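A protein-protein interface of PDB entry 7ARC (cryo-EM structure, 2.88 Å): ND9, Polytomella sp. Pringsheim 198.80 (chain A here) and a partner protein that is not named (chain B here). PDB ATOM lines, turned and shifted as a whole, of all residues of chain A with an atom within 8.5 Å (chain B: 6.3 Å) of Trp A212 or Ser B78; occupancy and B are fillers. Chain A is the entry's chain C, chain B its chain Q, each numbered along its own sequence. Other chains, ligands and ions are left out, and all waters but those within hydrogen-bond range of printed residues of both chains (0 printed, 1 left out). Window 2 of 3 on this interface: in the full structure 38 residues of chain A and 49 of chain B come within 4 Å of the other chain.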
ATOM      1  N   SER A 209      27.979  25.389  10.734  1.00  0.00           N
ATOM      2  CA  SER A 209      27.520  26.078  11.931  1.00  0.00           C
ATOM      3  C   SER A 209      26.035  25.834  12.153  1.00  0.00           C
ATOM      4  O   SER A 209      25.235  25.846  11.215  1.00  0.00           O
ATOM      5  CB  SER A 209      27.791  27.577  11.816  1.00  0.00           C
ATOM      6  OG  SER A 209      27.164  28.116  10.668  1.00  0.00           O
ATOM      7  N   SER A 210      25.670  25.614  13.413  1.00  0.00           N
ATOM      8  CA  SER A 210      24.320  25.425  13.916  1.00  0.00           C
ATOM      9  C   SER A 210      23.770  26.719  14.499  1.00  0.00           C
ATOM     10  O   SER A 210      24.500  27.466  15.151  1.00  0.00           O
ATOM     11  CB  SER A 210      24.298  24.344  14.994  1.00  0.00           C
ATOM     12  OG  SER A 210      22.996  24.183  15.520  1.00  0.00           O
ATOM     13  N   PRO A 211      22.494  27.023  14.265  1.00  0.00           N
ATOM     14  CA  PRO A 211      21.883  28.159  14.968  1.00  0.00           C
ATOM     15  C   PRO A 211      21.837  27.970  16.471  1.00  0.00           C
ATOM     16  O   PRO A 211      21.978  28.945  17.217  1.00  0.00           O
ATOM     17  CB  PRO A 211      20.476  28.229  14.359  1.00  0.00           C
ATOM     18  CG  PRO A 211      20.233  26.872  13.806  1.00  0.00           C
ATOM     19  CD  PRO A 211      21.561  26.396  13.320  1.00  0.00           C
ATOM     20  N   TRP A 212      21.644  26.740  16.944  1.00  0.00           N
ATOM     21  CA  TRP A 212      21.436  26.495  18.364  1.00  0.00           C
ATOM     22  C   TRP A 212      22.717  26.527  19.187  1.00  0.00           C
ATOM     23  O   TRP A 212      22.631  26.511  20.419  1.00  0.00           O
ATOM     24  CB  TRP A 212      20.739  25.148  18.556  1.00  0.00           C
ATOM     25  CG  TRP A 212      19.348  25.136  18.019  1.00  0.00           C
ATOM     26  CD1 TRP A 212      18.938  24.638  16.819  1.00  0.00           C
ATOM     27  CD2 TRP A 212      18.179  25.661  18.655  1.00  0.00           C
ATOM     28  NE1 TRP A 212      17.586  24.812  16.669  1.00  0.00           N
ATOM     29  CE2 TRP A 212      17.096  25.440  17.784  1.00  0.00           C
ATOM     30  CE3 TRP A 212      17.942  26.295  19.878  1.00  0.00           C
ATOM     31  CZ2 TRP A 212      15.796  25.828  18.096  1.00  0.00           C
ATOM     32  CZ3 TRP A 212      16.650  26.677  20.186  1.00  0.00           C
ATOM     33  CH2 TRP A 212      15.595  26.444  19.299  1.00  0.00           C
ATOM     34  N   ASP A 213      23.888  26.560  18.558  1.00  0.00           N
ATOM     35  CA  ASP A 213      25.128  26.556  19.322  1.00  0.00           C
ATOM     36  C   ASP A 213      25.266  27.841  20.133  1.00  0.00           C
ATOM     37  O   ASP A 213      24.763  28.903  19.755  1.00  0.00           O
ATOM     38  CB  ASP A 213      26.342  26.333  18.407  1.00  0.00           C
ATOM     39  CG  ASP A 213      26.545  27.436  17.369  1.00  0.00           C
ATOM     40  OD1 ASP A 213      26.943  27.093  16.237  1.00  0.00           O
ATOM     41  OD2 ASP A 213      26.351  28.632  17.665  1.00  0.00           O
ATOM     42  N   THR A 214      25.927  27.727  21.285  1.00  0.00           N
ATOM     43  CA  THR A 214      26.150  28.872  22.154  1.00  0.00           C
ATOM     44  C   THR A 214      27.617  29.167  22.421  1.00  0.00           C
ATOM     45  O   THR A 214      27.928  30.273  22.875  1.00  0.00           O
ATOM     46  CB  THR A 214      25.448  28.665  23.505  1.00  0.00           C
ATOM     47  OG1 THR A 214      25.990  27.507  24.153  1.00  0.00           O
ATOM     48  CG2 THR A 214      23.954  28.477  23.312  1.00  0.00           C
ATOM     49  N   LEU A 215      28.519  28.219  22.165  1.00  0.00           N
ATOM     50  CA  LEU A 215      29.921  28.398  22.515  1.00  0.00           C
ATOM     51  C   LEU A 215      30.625  29.422  21.635  1.00  0.00           C
ATOM     52  O   LEU A 215      31.653  29.965  22.046  1.00  0.00           O
ATOM     53  CB  LEU A 215      30.652  27.060  22.420  1.00  0.00           C
ATOM     54  CG  LEU A 215      30.661  26.175  23.664  1.00  0.00           C
ATOM     55  CD1 LEU A 215      31.367  24.867  23.365  1.00  0.00           C
ATOM     56  CD2 LEU A 215      31.318  26.886  24.829  1.00  0.00           C
ATOM     57  N   SER A 216      30.123  29.662  20.427  1.00  0.00           N
ATOM     58  CA  SER A 216      30.750  30.612  19.514  1.00  0.00           C
ATOM     59  C   SER A 216      30.725  32.037  20.053  1.00  0.00           C
ATOM     60  O   SER A 216      29.653  32.610  20.267  1.00  0.00           O
ATOM     61  CB  SER A 216      30.053  30.552  18.157  1.00  0.00           C
ATOM     62  OG  SER A 216      30.378  29.358  17.471  1.00  0.00           O
ATOM     63  N   LYS B  73      18.057  34.256   8.842  1.00  0.00           N
ATOM     64  CA  LYS B  73      17.852  32.934   9.414  1.00  0.00           C
ATOM     65  C   LYS B  73      17.401  31.955   8.339  1.00  0.00           C
ATOM     66  O   LYS B  73      16.589  32.288   7.473  1.00  0.00           O
ATOM     67  CB  LYS B  73      16.810  32.986  10.530  1.00  0.00           C
ATOM     68  CG  LYS B  73      16.577  31.647  11.208  1.00  0.00           C
ATOM     69  CD  LYS B  73      15.637  31.758  12.392  1.00  0.00           C
ATOM     70  CE  LYS B  73      14.204  31.974  11.947  1.00  0.00           C
ATOM     71  NZ  LYS B  73      13.267  31.965  13.105  1.00  0.00           N
ATOM     72  N   ALA B  74      17.939  30.740   8.393  1.00  0.00           N
ATOM     73  CA  ALA B  74      17.455  29.684   7.519  1.00  0.00           C
ATOM     74  C   ALA B  74      16.028  29.320   7.902  1.00  0.00           C
ATOM     75  O   ALA B  74      15.691  29.225   9.084  1.00  0.00           O
ATOM     76  CB  ALA B  74      18.360  28.458   7.611  1.00  0.00           C
ATOM     77  N   ALA B  75      15.184  29.115   6.890  1.00  0.00           N
ATOM     78  CA  ALA B  75      13.780  28.824   7.145  1.00  0.00           C
ATOM     79  C   ALA B  75      13.560  27.436   7.730  1.00  0.00           C
ATOM     80  O   ALA B  75      12.529  27.208   8.370  1.00  0.00           O
ATOM     81  CB  ALA B  75      12.973  28.976   5.855  1.00  0.00           C
ATOM     82  N   SER B  76      14.495  26.509   7.524  1.00  0.00           N
ATOM     83  CA  SER B  76      14.325  25.159   8.051  1.00  0.00           C
ATOM     84  C   SER B  76      14.395  25.134   9.574  1.00  0.00           C
ATOM     85  O   SER B  76      13.641  24.402  10.223  1.00  0.00           O
ATOM     86  CB  SER B  76      15.377  24.229   7.451  1.00  0.00           C
ATOM     87  OG  SER B  76      16.683  24.625   7.832  1.00  0.00           O
ATOM     88  N   GLN B  77      15.291  25.922  10.159  1.00  0.00           N
ATOM     89  CA  GLN B  77      15.568  25.887  11.586  1.00  0.00           C
ATOM     90  C   GLN B  77      15.012  27.119  12.286  1.00  0.00           C
ATOM     91  O   GLN B  77      14.836  28.177  11.677  1.00  0.00           O
ATOM     92  CB  GLN B  77      17.071  25.766  11.835  1.00  0.00           C
ATOM     93  CG  GLN B  77      17.626  24.433  11.389  1.00  0.00           C
ATOM     94  CD  GLN B  77      19.039  24.189  11.855  1.00  0.00           C
ATOM     95  OE1 GLN B  77      19.991  24.702  11.273  1.00  0.00           O
ATOM     96  NE2 GLN B  77      19.186  23.416  12.924  1.00  0.00           N
ATOM     97  N   SER B  78      14.733  26.965  13.580  1.00  0.00           N
ATOM     98  CA  SER B  78      14.178  28.029  14.406  1.00  0.00           C
ATOM     99  C   SER B  78      15.183  28.608  15.393  1.00  0.00           C
ATOM    100  O   SER B  78      14.806  29.437  16.226  1.00  0.00           O
ATOM    101  CB  SER B  78      12.945  27.523  15.157  1.00  0.00           C
ATOM    102  OG  SER B  78      11.909  27.177  14.255  1.00  0.00           O
ATOM    103  N   GLY B  79      16.445  28.193  15.332  1.00  0.00           N
ATOM    104  CA  GLY B  79      17.449  28.786  16.191  1.00  0.00           C
ATOM    105  C   GLY B  79      17.780  30.207  15.778  1.00  0.00           C
ATOM    106  O   GLY B  79      17.749  30.564  14.601  1.00  0.00           O
ATOM    107  N   LEU B  80      18.105  31.030  16.773  1.00  0.00           N
ATOM    108  CA  LEU B  80      18.400  32.443  16.567  1.00  0.00           C
ATOM    109  C   LEU B  80      19.887  32.762  16.644  1.00  0.00           C
ATOM    110  O   LEU B  80      20.251  33.942  16.666  1.00  0.00           O
ATOM    111  CB  LEU B  80      17.642  33.299  17.584  1.00  0.00           C
ATOM    112  CG  LEU B  80      16.183  33.686  17.321  1.00  0.00           C
ATOM    113  CD1 LEU B  80      16.080  34.564  16.087  1.00  0.00           C
ATOM    114  CD2 LEU B  80      15.274  32.476  17.201  1.00  0.00           C
ATOM    115  N   GLY B  81      20.753  31.750  16.701  1.00  0.00           N
ATOM    116  CA  GLY B  81      22.174  32.020  16.855  1.00  0.00           C
ATOM    117  C   GLY B  81      22.762  32.774  15.679  1.00  0.00           C
ATOM    118  O   GLY B  81      23.514  33.735  15.854  1.00  0.00           O
ATOM    119  N   ARG B  82      22.434  32.343  14.460  1.00  0.00           N
ATOM    120  CA  ARG B  82      23.016  32.967  13.278  1.00  0.00           C
ATOM    121  C   ARG B  82      22.494  34.384  13.065  1.00  0.00           C
ATOM    122  O   ARG B  82      23.175  35.204  12.440  1.00  0.00           O
ATOM    123  CB  ARG B  82      22.729  32.111  12.046  1.00  0.00           C
ATOM    124  CG  ARG B  82      23.367  30.725  12.051  1.00  0.00           C
ATOM    125  CD  ARG B  82      24.888  30.762  11.994  1.00  0.00           C
ATOM    126  NE  ARG B  82      25.508  30.893  13.307  1.00  0.00           N
ATOM    127  CZ  ARG B  82      26.786  31.190  13.502  1.00  0.00           C
ATOM    128  NH1 ARG B  82      27.610  31.395  12.490  1.00  0.00           N
ATOM    129  NH2 ARG B  82      27.247  31.279  14.747  1.00  0.00           N
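Printed residues of chain B within 4 Å of Ser A209: Arg B82. Printed residues of chain B within 4 Å of Pro A211: Gln B77 (3.1 Å), Gly B79 (3.6 Å) and Gly B81 (3.1 Å). Leu A215 touches none of the printed residues of chain B. Printed residues of chain A within 4 Å of Gln B77: Pro A211 (3.1 Å). Ser B78 touches one residue of chain A. Of the printed residues of chain A, Gly B79 touches Pro A211 (3.6 Å) and Trp A212 (3.7 Å). Leu B80 touches none of the printed residues of chain A. Of the printed residues of chain A, Gly B81 touches Pro A211. Printed residues of chain A within 4 Å of Arg B82: Ser A209 (3.7 Å). The nearest printed residue of chain B that does not touch Pro A211 is Arg B82 (4.2 Å).
The side-chain hydroxyl of Ser A210 lies within hydrogen-bond range of the backbone NH of Trp A212 (3.2 Å).
Of the 10 printed residues of chain B, 5 touch a printed residue of chain A. Of the 8 printed residues of chain A, 3 touch a printed residue of chain B. Printed residues of chain A that touch a printed residue of chain B: Ser A209, Pro A211 and Trp A212. Hydrophobic or aromatic side chains of chain A within 4 Å of the printed part of chain B: Pro A211 and Trp A212. Among the printed residues, 6 pairs touch across the chains.
O of Pro A211 sits close to N of Gly B81, at 3.1 Å.
CD of Arg B82 touches OG of Ser A209, at 3.7 Å. CD of Pro A211 touches OE1 of Gln B77 (3.1 Å). Pro A211 touches Gly B79 (CB to CA, 3.6 Å). C of Ser B78 touches CZ2 of Trp A212 (3.9 Å). CZ2 of Trp A212 touches N of Gly B79, at 3.7 Å.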
